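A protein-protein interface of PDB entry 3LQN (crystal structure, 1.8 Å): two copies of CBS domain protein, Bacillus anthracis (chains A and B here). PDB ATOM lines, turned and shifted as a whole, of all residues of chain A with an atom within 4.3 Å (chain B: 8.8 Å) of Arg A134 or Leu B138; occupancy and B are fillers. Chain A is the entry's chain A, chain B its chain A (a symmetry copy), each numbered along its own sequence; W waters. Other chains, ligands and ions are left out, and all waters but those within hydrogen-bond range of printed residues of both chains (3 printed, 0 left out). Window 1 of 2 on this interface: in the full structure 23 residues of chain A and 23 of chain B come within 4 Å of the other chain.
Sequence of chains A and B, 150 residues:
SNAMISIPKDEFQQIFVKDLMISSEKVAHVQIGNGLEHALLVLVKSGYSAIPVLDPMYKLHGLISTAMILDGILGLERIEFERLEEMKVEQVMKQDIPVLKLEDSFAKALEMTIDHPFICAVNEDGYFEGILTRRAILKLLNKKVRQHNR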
ATOM      1  N   LEU A 110      -1.701  29.875  15.182  1.00  0.00           N
ATOM      2  CA  LEU A 110      -0.736  29.352  16.155  1.00  0.00           C
ATOM      3  C   LEU A 110      -1.290  29.404  17.569  1.00  0.00           C
ATOM      4  O   LEU A 110      -1.246  28.423  18.302  1.00  0.00           O
ATOM      5  CB  LEU A 110       0.560  30.153  16.112  1.00  0.00           C
ATOM      6  CG  LEU A 110       1.516  29.912  17.301  1.00  0.00           C
ATOM      7  CD1 LEU A 110       1.997  28.485  17.332  1.00  0.00           C
ATOM      8  CD2 LEU A 110       2.662  30.854  17.140  1.00  0.00           C
ATOM      9  N   THR A 113      -4.099  26.861  18.073  1.00  0.00           N
ATOM     10  CA  THR A 113      -3.687  25.456  18.095  1.00  0.00           C
ATOM     11  C   THR A 113      -3.098  25.000  19.452  1.00  0.00           C
ATOM     12  O   THR A 113      -2.995  23.799  19.696  1.00  0.00           O
ATOM     13  CB  THR A 113      -2.682  25.040  16.994  1.00  0.00           C
ATOM     14  OG1 THR A 113      -1.479  25.822  17.120  1.00  0.00           O
ATOM     15  CG2 THR A 113      -3.273  25.191  15.643  1.00  0.00           C
ATOM     16  N   ILE A 114      -2.728  25.933  20.321  1.00  0.00           N
ATOM     17  CA  ILE A 114      -2.267  25.520  21.655  1.00  0.00           C
ATOM     18  C   ILE A 114      -3.292  24.607  22.380  1.00  0.00           C
ATOM     19  O   ILE A 114      -2.933  23.534  22.858  1.00  0.00           O
ATOM     20  CB  ILE A 114      -1.786  26.708  22.471  1.00  0.00           C
ATOM     21  CG1 ILE A 114      -0.569  27.315  21.759  1.00  0.00           C
ATOM     22  CG2 ILE A 114      -1.391  26.261  23.850  1.00  0.00           C
ATOM     23  CD1 ILE A 114      -0.528  28.777  21.817  1.00  0.00           C
ATOM     24  N   ASP A 115      -4.575  24.974  22.377  1.00  0.00           N
ATOM     25  CA  ASP A 115      -5.587  24.134  23.028  1.00  0.00           C
ATOM     26  C   ASP A 115      -6.449  23.311  22.063  1.00  0.00           C
ATOM     27  O   ASP A 115      -7.200  22.439  22.488  1.00  0.00           O
ATOM     28  CB  ASP A 115      -6.500  24.983  23.911  1.00  0.00           C
ATOM     29  CG  ASP A 115      -5.769  25.600  25.073  1.00  0.00           C
ATOM     30  OD1 ASP A 115      -4.830  24.955  25.578  1.00  0.00           O
ATOM     31  OD2 ASP A 115      -6.137  26.723  25.479  1.00  0.00           O
ATOM     32  N   HIS A 116      -6.347  23.575  20.763  1.00  0.00           N
ATOM     33  CA  HIS A 116      -7.220  22.874  19.813  1.00  0.00           C
ATOM     34  C   HIS A 116      -6.395  22.207  18.738  1.00  0.00           C
ATOM     35  O   HIS A 116      -5.813  22.892  17.907  1.00  0.00           O
ATOM     36  CB  HIS A 116      -8.228  23.867  19.221  1.00  0.00           C
ATOM     37  CG  HIS A 116      -8.881  24.734  20.250  1.00  0.00           C
ATOM     38  ND1 HIS A 116      -9.972  24.330  20.988  1.00  0.00           N
ATOM     39  CD2 HIS A 116      -8.572  25.976  20.704  1.00  0.00           C
ATOM     40  CE1 HIS A 116     -10.329  25.285  21.822  1.00  0.00           C
ATOM     41  NE2 HIS A 116      -9.486  26.298  21.670  1.00  0.00           N
ATOM     42  N   PRO A 117      -6.352  20.885  18.732  1.00  0.00           N
ATOM     43  CA  PRO A 117      -5.523  20.048  17.863  1.00  0.00           C
ATOM     44  C   PRO A 117      -5.963  20.247  16.414  1.00  0.00           C
ATOM     45  O   PRO A 117      -5.211  20.065  15.473  1.00  0.00           O
ATOM     46  CB  PRO A 117      -5.840  18.650  18.332  1.00  0.00           C
ATOM     47  CG  PRO A 117      -6.309  18.837  19.745  1.00  0.00           C
ATOM     48  CD  PRO A 117      -7.102  20.072  19.701  1.00  0.00           C
ATOM     49  N   THR A 133      -4.294  21.922  11.085  1.00  0.00           N
ATOM     50  CA  THR A 133      -3.760  21.031  12.110  1.00  0.00           C
ATOM     51  C   THR A 133      -2.583  21.663  12.809  1.00  0.00           C
ATOM     52  O   THR A 133      -1.907  22.592  12.326  1.00  0.00           O
ATOM     53  CB  THR A 133      -3.169  19.782  11.500  1.00  0.00           C
ATOM     54  OG1 THR A 133      -2.069  20.199  10.682  1.00  0.00           O
ATOM     55  CG2 THR A 133      -4.197  19.076  10.657  1.00  0.00           C
ATOM     56  N   ARG A 134      -2.248  21.067  13.948  1.00  0.00           N
ATOM     57  CA  ARG A 134      -1.036  21.441  14.625  1.00  0.00           C
ATOM     58  C   ARG A 134       0.201  21.164  13.818  1.00  0.00           C
ATOM     59  O   ARG A 134       1.134  21.947  13.853  1.00  0.00           O
ATOM     60  CB  ARG A 134      -0.905  20.682  15.955  1.00  0.00           C
ATOM     61  CG  ARG A 134      -1.883  21.171  16.941  1.00  0.00           C
ATOM     62  CD  ARG A 134      -1.741  20.326  18.155  1.00  0.00           C
ATOM     63  NE  ARG A 134      -2.314  20.992  19.297  1.00  0.00           N
ATOM     64  CZ  ARG A 134      -2.580  20.358  20.418  1.00  0.00           C
ATOM     65  NH1 ARG A 134      -2.317  19.066  20.487  1.00  0.00           N
ATOM     66  NH2 ARG A 134      -3.115  21.009  21.430  1.00  0.00           N
ATOM     67  N   ARG A 135       0.242  20.047  13.103  1.00  0.00           N
ATOM     68  CA  ARG A 135       1.456  19.735  12.352  1.00  0.00           C
ATOM     69  C   ARG A 135       1.867  20.862  11.417  1.00  0.00           C
ATOM     70  O   ARG A 135       3.020  21.264  11.408  1.00  0.00           O
ATOM     71  CB  ARG A 135       1.323  18.425  11.584  1.00  0.00           C
ATOM     72  CG  ARG A 135       2.531  18.141  10.734  1.00  0.00           C
ATOM     73  CD  ARG A 135       2.491  16.740  10.166  1.00  0.00           C
ATOM     74  NE  ARG A 135       3.758  16.414   9.526  1.00  0.00           N
ATOM     75  CZ  ARG A 135       4.105  16.809   8.307  1.00  0.00           C
ATOM     76  NH1 ARG A 135       3.280  17.550   7.578  1.00  0.00           N
ATOM     77  NH2 ARG A 135       5.281  16.460   7.818  1.00  0.00           N
ATOM     78  N   ALA A 136       0.911  21.394  10.649  1.00  0.00           N
ATOM     79  CA  ALA A 136       1.212  22.454   9.734  1.00  0.00           C
ATOM     80  C   ALA A 136       1.840  23.665  10.458  1.00  0.00           C
ATOM     81  O   ALA A 136       2.816  24.245   9.996  1.00  0.00           O
ATOM     82  CB  ALA A 136      -0.085  22.874   8.922  1.00  0.00           C
ATOM     83  N   ILE A 137       1.279  24.056  11.598  1.00  0.00           N
ATOM     84  CA  ILE A 137       1.899  25.149  12.351  1.00  0.00           C
ATOM     85  C   ILE A 137       3.332  24.822  12.824  1.00  0.00           C
ATOM     86  O   ILE A 137       4.251  25.667  12.769  1.00  0.00           O
ATOM     87  CB  ILE A 137       0.999  25.607  13.518  1.00  0.00           C
ATOM     88  CG1 ILE A 137      -0.090  26.545  12.993  1.00  0.00           C
ATOM     89  CG2 ILE A 137       1.803  26.391  14.516  1.00  0.00           C
ATOM     90  CD1 ILE A 137      -1.264  25.874  12.403  1.00  0.00           C
ATOM     91  N   LEU A 138       3.530  23.582  13.244  1.00  0.00           N
ATOM     92  CA  LEU A 138       4.803  23.155  13.808  1.00  0.00           C
ATOM     93  C   LEU A 138       5.835  22.972  12.712  1.00  0.00           C
ATOM     94  O   LEU A 138       7.013  23.232  12.908  1.00  0.00           O
ATOM     95  CB  LEU A 138       4.642  21.851  14.605  1.00  0.00           C
ATOM     96  CG  LEU A 138       3.977  21.964  15.977  1.00  0.00           C
ATOM     97  CD1 LEU A 138       3.316  20.616  16.395  1.00  0.00           C
ATOM     98  CD2 LEU A 138       4.932  22.438  17.036  1.00  0.00           C
ATOM     99  N   LEU B  20       9.549  19.779  30.005  1.00  0.00           N
ATOM    100  CA  LEU B  20       8.335  19.960  29.216  1.00  0.00           C
ATOM    101  C   LEU B  20       7.378  18.764  29.389  1.00  0.00           C
ATOM    102  O   LEU B  20       6.182  18.846  29.069  1.00  0.00           O
ATOM    103  CB  LEU B  20       8.683  20.009  27.717  1.00  0.00           C
ATOM    104  CG  LEU B  20       9.483  21.185  27.115  1.00  0.00           C
ATOM    105  CD1 LEU B  20       9.795  20.976  25.645  1.00  0.00           C
ATOM    106  CD2 LEU B  20       8.743  22.471  27.282  1.00  0.00           C
ATOM    107  N   SER B  49      -5.319   9.745  24.054  1.00  0.00           N
ATOM    108  CA  SER B  49      -5.636   9.106  22.800  1.00  0.00           C
ATOM    109  C   SER B  49      -4.623   8.014  22.585  1.00  0.00           C
ATOM    110  O   SER B  49      -4.841   7.125  21.766  1.00  0.00           O
ATOM    111  CB  SER B  49      -5.544  10.099  21.641  1.00  0.00           C
ATOM    112  OG  SER B  49      -4.271  10.727  21.694  1.00  0.00           O
ATOM    113  N   PHE B 106      15.327  20.816  23.594  1.00  0.00           N
ATOM    114  CA  PHE B 106      14.075  21.329  23.061  1.00  0.00           C
ATOM    115  C   PHE B 106      14.051  21.214  21.521  1.00  0.00           C
ATOM    116  O   PHE B 106      13.060  20.818  20.927  1.00  0.00           O
ATOM    117  CB  PHE B 106      13.863  22.777  23.487  1.00  0.00           C
ATOM    118  CG  PHE B 106      12.658  23.393  22.844  1.00  0.00           C
ATOM    119  CD1 PHE B 106      11.406  23.214  23.399  1.00  0.00           C
ATOM    120  CD2 PHE B 106      12.773  24.083  21.642  1.00  0.00           C
ATOM    121  CE1 PHE B 106      10.295  23.743  22.792  1.00  0.00           C
ATOM    122  CE2 PHE B 106      11.670  24.629  21.035  1.00  0.00           C
ATOM    123  CZ  PHE B 106      10.423  24.457  21.606  1.00  0.00           C
ATOM    124  N   LEU B 110      11.082  19.444  19.479  1.00  0.00           N
ATOM    125  CA  LEU B 110      10.311  20.195  18.483  1.00  0.00           C
ATOM    126  C   LEU B 110      10.311  19.491  17.136  1.00  0.00           C
ATOM    127  O   LEU B 110       9.268  19.298  16.524  1.00  0.00           O
ATOM    128  CB  LEU B 110      10.887  21.594  18.299  1.00  0.00           C
ATOM    129  CG  LEU B 110      10.373  22.354  17.057  1.00  0.00           C
ATOM    130  CD1 LEU B 110       8.889  22.603  17.148  1.00  0.00           C
ATOM    131  CD2 LEU B 110      11.123  23.642  16.989  1.00  0.00           C
ATOM    132  N   THR B 113       8.230  16.286  17.224  1.00  0.00           N
ATOM    133  CA  THR B 113       6.782  16.472  17.327  1.00  0.00           C
ATOM    134  C   THR B 113       6.100  16.819  15.982  1.00  0.00           C
ATOM    135  O   THR B 113       4.881  16.707  15.873  1.00  0.00           O
ATOM    136  CB  THR B 113       6.318  17.525  18.363  1.00  0.00           C
ATOM    137  OG1 THR B 113       6.874  18.810  18.024  1.00  0.00           O
ATOM    138  CG2 THR B 113       6.701  17.129  19.739  1.00  0.00           C
ATOM    139  N   ILE B 114       6.867  17.222  14.975  1.00  0.00           N
ATOM    140  CA  ILE B 114       6.250  17.452  13.660  1.00  0.00           C
ATOM    141  C   ILE B 114       5.451  16.220  13.156  1.00  0.00           C
ATOM    142  O   ILE B 114       4.290  16.352  12.775  1.00  0.00           O
ATOM    143  CB  ILE B 114       7.253  18.009  12.665  1.00  0.00           C
ATOM    144  CG1 ILE B 114       7.719  19.381  13.173  1.00  0.00           C
ATOM    145  CG2 ILE B 114       6.610  18.164  11.315  1.00  0.00           C
ATOM    146  CD1 ILE B 114       9.141  19.638  12.937  1.00  0.00           C
ATOM    147  N   ASP B 115       6.024  15.019  13.245  1.00  0.00           N
ATOM    148  CA  ASP B 115       5.301  13.820  12.804  1.00  0.00           C
ATOM    149  C   ASP B 115       4.734  12.963  13.941  1.00  0.00           C
ATOM    150  O   ASP B 115       3.960  12.041  13.702  1.00  0.00           O
ATOM    151  CB  ASP B 115       6.196  12.949  11.923  1.00  0.00           C
ATOM    152  CG  ASP B 115       6.563  13.623  10.628  1.00  0.00           C
ATOM    153  OD1 ASP B 115       5.724  14.385  10.111  1.00  0.00           O
ATOM    154  OD2 ASP B 115       7.685  13.385  10.130  1.00  0.00           O
ATOM    155  N   PRO B 117       2.674  13.081  17.511  1.00  0.00           N
ATOM    156  CA  PRO B 117       1.804  13.870  18.385  1.00  0.00           C
ATOM    157  C   PRO B 117       2.219  13.640  19.837  1.00  0.00           C
ATOM    158  O   PRO B 117       2.011  14.462  20.712  1.00  0.00           O
ATOM    159  CB  PRO B 117       0.438  13.288  18.120  1.00  0.00           C
ATOM    160  CG  PRO B 117       0.557  12.689  16.749  1.00  0.00           C
ATOM    161  CD  PRO B 117       1.904  12.105  16.725  1.00  0.00           C
ATOM    162  N   PHE B 118       2.802  12.493  20.079  1.00  0.00           N
ATOM    163  CA  PHE B 118       3.442  12.334  21.352  1.00  0.00           C
ATOM    164  C   PHE B 118       4.481  11.259  21.499  1.00  0.00           C
ATOM    165  O   PHE B 118       4.502  10.193  20.857  1.00  0.00           O
ATOM    166  CB  PHE B 118       2.494  12.523  22.555  1.00  0.00           C
ATOM    167  CG  PHE B 118       2.021  11.252  23.208  1.00  0.00           C
ATOM    168  CD1 PHE B 118       2.928  10.351  23.774  1.00  0.00           C
ATOM    169  CD2 PHE B 118       0.662  11.007  23.338  1.00  0.00           C
ATOM    170  CE1 PHE B 118       2.473   9.186  24.406  1.00  0.00           C
ATOM    171  CE2 PHE B 118       0.213   9.894  23.977  1.00  0.00           C
ATOM    172  CZ  PHE B 118       1.127   8.970  24.523  1.00  0.00           C
ATOM    173  N   LEU B 132       5.823  13.616  26.156  1.00  0.00           N
ATOM    174  CA  LEU B 132       5.996  14.993  25.718  1.00  0.00           C
ATOM    175  C   LEU B 132       5.068  15.255  24.535  1.00  0.00           C
ATOM    176  O   LEU B 132       5.217  14.654  23.484  1.00  0.00           O
ATOM    177  CB  LEU B 132       7.457  15.268  25.369  1.00  0.00           C
ATOM    178  CG  LEU B 132       7.960  16.554  24.733  1.00  0.00           C
ATOM    179  CD1 LEU B 132       8.099  17.667  25.737  1.00  0.00           C
ATOM    180  CD2 LEU B 132       9.281  16.206  24.173  1.00  0.00           C
ATOM    181  N   THR B 133       4.123  16.167  24.733  1.00  0.00           N
ATOM    182  CA  THR B 133       3.057  16.433  23.773  1.00  0.00           C
ATOM    183  C   THR B 133       3.413  17.601  22.887  1.00  0.00           C
ATOM    184  O   THR B 133       4.261  18.464  23.187  1.00  0.00           O
ATOM    185  CB  THR B 133       1.797  16.894  24.463  1.00  0.00           C
ATOM    186  OG1 THR B 133       2.105  18.133  25.111  1.00  0.00           O
ATOM    187  CG2 THR B 133       1.359  15.877  25.484  1.00  0.00           C
ATOM    188  N   ARG B 134       2.657  17.704  21.800  1.00  0.00           N
ATOM    189  CA  ARG B 134       2.755  18.869  20.964  1.00  0.00           C
ATOM    190  C   ARG B 134       2.360  20.136  21.670  1.00  0.00           C
ATOM    191  O   ARG B 134       2.970  21.167  21.447  1.00  0.00           O
ATOM    192  CB  ARG B 134       1.855  18.723  19.728  1.00  0.00           C
ATOM    193  CG  ARG B 134       2.397  17.722  18.794  1.00  0.00           C
ATOM    194  CD  ARG B 134       1.421  17.587  17.681  1.00  0.00           C
ATOM    195  NE  ARG B 134       2.054  16.992  16.532  1.00  0.00           N
ATOM    196  CZ  ARG B 134       1.363  16.500  15.526  1.00  0.00           C
ATOM    197  NH1 ARG B 134       0.045  16.553  15.585  1.00  0.00           N
ATOM    198  NH2 ARG B 134       1.987  15.955  14.504  1.00  0.00           N
ATOM    199  N   ARG B 135       1.330  20.090  22.504  1.00  0.00           N
ATOM    200  CA  ARG B 135       0.899  21.323  23.160  1.00  0.00           C
ATOM    201  C   ARG B 135       2.030  22.010  23.908  1.00  0.00           C
ATOM    202  O   ARG B 135       2.235  23.203  23.753  1.00  0.00           O
ATOM    203  CB  ARG B 135      -0.287  21.082  24.088  1.00  0.00           C
ATOM    204  CG  ARG B 135      -0.680  22.325  24.840  1.00  0.00           C
ATOM    205  CD  ARG B 135      -1.990  22.138  25.570  1.00  0.00           C
ATOM    206  NE  ARG B 135      -2.455  23.407  26.113  1.00  0.00           N
ATOM    207  CZ  ARG B 135      -2.002  23.953  27.236  1.00  0.00           C
ATOM    208  NH1 ARG B 135      -1.065  23.344  27.951  1.00  0.00           N
ATOM    209  NH2 ARG B 135      -2.490  25.111  27.641  1.00  0.00           N
ATOM    210  N   ALA B 136       2.788  21.245  24.700  1.00  0.00           N
ATOM    211  CA  ALA B 136       3.870  21.810  25.448  1.00  0.00           C
ATOM    212  C   ALA B 136       4.882  22.526  24.526  1.00  0.00           C
ATOM    213  O   ALA B 136       5.335  23.628  24.814  1.00  0.00           O
ATOM    214  CB  ALA B 136       4.580  20.699  26.331  1.00  0.00           C
ATOM    215  N   ILE B 137       5.243  21.900  23.410  1.00  0.00           N
ATOM    216  CA  ILE B 137       6.136  22.587  22.473  1.00  0.00           C
ATOM    217  C   ILE B 137       5.531  23.887  21.900  1.00  0.00           C
ATOM    218  O   ILE B 137       6.213  24.924  21.761  1.00  0.00           O
ATOM    219  CB  ILE B 137       6.617  21.635  21.357  1.00  0.00           C
ATOM    220  CG1 ILE B 137       7.770  20.773  21.874  1.00  0.00           C
ATOM    221  CG2 ILE B 137       7.152  22.426  20.197  1.00  0.00           C
ATOM    222  CD1 ILE B 137       7.366  19.589  22.656  1.00  0.00           C
ATOM    223  N   LEU B 138       4.239  23.841  21.613  1.00  0.00           N
ATOM    224  CA  LEU B 138       3.553  24.957  20.977  1.00  0.00           C
ATOM    225  C   LEU B 138       3.313  26.071  21.978  1.00  0.00           C
ATOM    226  O   LEU B 138       3.353  27.244  21.635  1.00  0.00           O
ATOM    227  CB  LEU B 138       2.219  24.504  20.362  1.00  0.00           C
ATOM    228  CG  LEU B 138       2.302  23.706  19.060  1.00  0.00           C
ATOM    229  CD1 LEU B 138       1.047  22.802  18.874  1.00  0.00           C
ATOM    230  CD2 LEU B 138       2.501  24.590  17.861  1.00  0.00           C
ATOM    231  N   LYS B 139       3.076  25.697  23.223  1.00  0.00           N
ATOM    232  CA  LYS B 139       2.751  26.683  24.229  1.00  0.00           C
ATOM    233  C   LYS B 139       4.019  27.515  24.449  1.00  0.00           C
ATOM    234  O   LYS B 139       3.974  28.740  24.519  1.00  0.00           O
ATOM    235  CB  LYS B 139       2.266  25.964  25.483  1.00  0.00           C
ATOM    236  CG  LYS B 139       1.744  26.860  26.571  1.00  0.00           C
ATOM    237  CD  LYS B 139       1.480  26.070  27.834  1.00  0.00           C
ATOM    238  CE  LYS B 139       2.160  26.734  29.027  1.00  0.00           C
ATOM    239  NZ  LYS B 139       2.290  25.813  30.193  1.00  0.00           N
ATOM    240  N   LEU B 140       5.157  26.831  24.497  1.00  0.00           N
ATOM    241  CA  LEU B 140       6.443  27.481  24.610  1.00  0.00           C
ATOM    242  C   LEU B 140       6.767  28.358  23.395  1.00  0.00           C
ATOM    243  O   LEU B 140       7.284  29.451  23.556  1.00  0.00           O
ATOM    244  CB  LEU B 140       7.535  26.433  24.827  1.00  0.00           C
ATOM    245  CG  LEU B 140       8.905  27.023  25.127  1.00  0.00           C
ATOM    246  CD1 LEU B 140       8.779  28.062  26.210  1.00  0.00           C
ATOM    247  CD2 LEU B 140       9.855  25.930  25.554  1.00  0.00           C
ATOM    248  N   LEU B 141       6.458  27.865  22.201  1.00  0.00           N
ATOM    249  CA  LEU B 141       6.759  28.588  20.972  1.00  0.00           C
ATOM    250  C   LEU B 141       5.850  29.802  20.810  1.00  0.00           C
ATOM    251  O   LEU B 141       6.266  30.836  20.286  1.00  0.00           O
ATOM    252  CB  LEU B 141       6.622  27.665  19.759  1.00  0.00           C
ATOM    253  CG  LEU B 141       7.718  26.612  19.582  1.00  0.00           C
ATOM    254  CD1 LEU B 141       7.484  25.800  18.318  1.00  0.00           C
ATOM    255  CD2 LEU B 141       9.092  27.263  19.560  1.00  0.00           C
ATOM    256  N   ASN B 142       4.608  29.670  21.265  1.00  0.00           N
ATOM    257  CA  ASN B 142       3.610  30.716  21.081  1.00  0.00           C
ATOM    258  C   ASN B 142       4.019  32.026  21.747  1.00  0.00           C
ATOM    259  O   ASN B 142       4.021  33.081  21.114  1.00  0.00           O
ATOM    260  CB  ASN B 142       2.250  30.259  21.613  1.00  0.00           C
ATOM    261  CG  ASN B 142       1.176  31.318  21.454  1.00  0.00           C
ATOM    262  OD1 ASN B 142       1.063  31.950  20.404  1.00  0.00           O
ATOM    263  ND2 ASN B 142       0.380  31.514  22.498  1.00  0.00           N
ATOM    264  N   LYS B 143       4.365  31.950  23.028  1.00  0.00           N
ATOM    265  CA  LYS B 143       4.743  33.134  23.790  1.00  0.00           C
ATOM    266  C   LYS B 143       6.015  33.766  23.234  1.00  0.00           C
ATOM    267  O   LYS B 143       6.077  34.977  23.023  1.00  0.00           O
ATOM    268  CB  LYS B 143       4.933  32.782  25.268  1.00  0.00           C
ATOM    269  CG  LYS B 143       5.909  31.643  25.513  1.00  0.00           C
ATOM    270  CD  LYS B 143       6.166  31.447  26.999  1.00  0.00           C
ATOM    271  CE  LYS B 143       4.868  31.226  27.759  1.00  0.00           C
ATOM    272  NZ  LYS B 143       4.209  32.512  28.118  1.00  0.00           N
ATOM    273  N   LYS B 144       7.028  32.937  23.001  1.00  0.00           N
ATOM    274  CA  LYS B 144       8.354  33.429  22.650  1.00  0.00           C
ATOM    275  C   LYS B 144       8.323  34.212  21.341  1.00  0.00           C
ATOM    276  O   LYS B 144       8.621  35.406  21.313  1.00  0.00           O
ATOM    277  CB  LYS B 144       9.346  32.269  22.545  1.00  0.00           C
ATOM    278  CG  LYS B 144      10.179  32.050  23.797  1.00  0.00           C
ATOM    279  CD  LYS B 144      11.043  30.805  23.675  1.00  0.00           C
ATOM    280  CE  LYS B 144      11.827  30.550  24.951  1.00  0.00           C
ATOM    281  NZ  LYS B 144      12.488  29.215  24.940  1.00  0.00           N
ATOM    282  N   VAL B 145       7.962  33.531  20.258  1.00  0.00           N
ATOM    283  CA  VAL B 145       7.876  34.169  18.939  1.00  0.00           C
ATOM    284  C   VAL B 145       7.152  35.538  18.917  1.00  0.00           C
ATOM    285  O   VAL B 145       7.568  36.495  18.226  1.00  0.00           O
ATOM    286  CB  VAL B 145       7.243  33.203  17.916  1.00  0.00           C
ATOM    287  CG1 VAL B 145       6.588  33.965  16.766  1.00  0.00           C
ATOM    288  CG2 VAL B 145       8.290  32.212  17.417  1.00  0.00           C
HETATM  289  O   HOH W   1      -0.847  17.959  22.763  1.00  0.00           O
HETATM  290  O   HOH W   2      -1.515  17.554  13.320  1.00  0.00           O
HETATM  291  O   HOH W   3      -1.837  16.985  18.121  1.00  0.00           O
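The backbone NH of Arg B135 lies close to the side-chain hydroxyl of Thr B133 (3.4 Å). The backbone carbonyl oxygen (O) of Ile A114 lies within hydrogen-bond range of the guanidinium group (NH2) of Arg A134, at 2.9 Å. OG1 of Thr A133 sits close to N of Arg A135 (3.4 Å). O of Thr B113 sits at hydrogen-bond distance from NE of Arg B134 (2.9 Å). The backbone carbonyl oxygen of Thr A113 sits at hydrogen-bond distance from the guanidinium group of Arg A134, 2.9 Å away. N of Arg A134 is in hydrogen-bond range of O of Pro A117, at 3.5 Å.
Ile A114 touches Leu B138, and with the chains exchanged Leu A138 touches Ile B114. Asp A115 touches Arg B135, and with the chains exchanged Arg A135 touches Asp B115. Arg A134 touches Arg B135, and with the chains exchanged Arg A135 touches Arg B134. Ile A137 touches Leu B138, and with the chains exchanged Leu A138 touches Ile B137. Positions printed for both chains: 110, 113, 114, 115, 117, 133, 134, 135, 136, 137 and 138.
NE of Arg B135 lies close to O of Ile A114. The guanidinium group (NE) of Arg A135 is in salt-bridge range of the side-chain carboxylate (OD1) of Asp B115, at 2.9 Å. The backbone carbonyl oxygen of Ile B114 sits close to the guanidinium group of Arg A135. OD1 of Asp A115 is in salt-bridge range of NE of Arg B135.
Of the 23 printed residues of chain B, 8 touch a printed residue of chain A. Printed residues of chain B that touch a printed residue of chain A: Leu B110, Ile B114, Asp B115, Arg B134, Arg B135, Ile B137, Leu B138 and Asn B142. Hydrophobic or aromatic side chains of chain B that line the printed part of chain A: Leu B110, Ile B114, Ile B137 and Leu B138. Of the 12 printed residues of chain A, 7 touch a printed residue of chain B. Printed residues of chain A that touch a printed residue of chain B: Leu A110, Ile A114, Asp A115, Arg A134, Arg A135, Ile A137 and Leu A138. Among the printed residues, 17 pairs touch across the chains. Among the printed residues, Asp or Glu carboxylates within 4 Å of a Lys or Arg side-chain nitrogen of the other chain: Asp A115 with Arg B135 (2.9 Å) and Arg A135 with Asp B115 (2.9 Å).
Leu A110 touches Leu B138. Leu A110 touches Asn B142. Leu B138 touches Ile A114 (O to CG1, 3.9 Å). Asn B142 touches Ile A114 (ND2 to CD1, 3.0 Å). Arg A134 touches Arg B135 (NH2 to CB, 3.9 Å). Arg A135 touches Arg B134 (CB to NH2, 3.9 Å). Ile A137 touches Leu B138. Leu A138 touches Ile B114. Arg B134 touches Leu A138. Leu B138 touches Leu A138.
No residue of chain B comes within 4 Å of Pro A117. No residue of chain B comes within 4 Å of Thr A133. Of the printed residues of chain B, Arg A134 touches Arg B135 and Leu B138. Printed residues of chain B within 4 Å of Ile A137: Leu B138. Printed residues of chain B within 4 Å of Leu A138: Leu B110, Ile B114, Arg B134, Ile B137 and Leu B138. Pro B117 touches none of the printed residues of chain A. Of chain A, only Leu A110, Ile A114, Arg A134, Ile A137 and Leu A138 come within 4 Å of Leu B138. Of the printed residues of chain A, Asn B142 touches Leu A110 (3.7 Å) and Ile A114 (3.0 Å). Lys B143 touches none of the printed residues of chain A. The nearest residue of chain A that does not touch Leu B138 is Thr A113 (4.2 Å).
Water W2 bridges NH1 of Arg B134 (2.9 Å) and N of Arg A135 (3.1 Å). Water W1 bridges the guanidinium group of Arg A134 and the backbone NH of Arg B135. Water W3 bridges NH1 of Arg B134 and NH1 of Arg A134.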
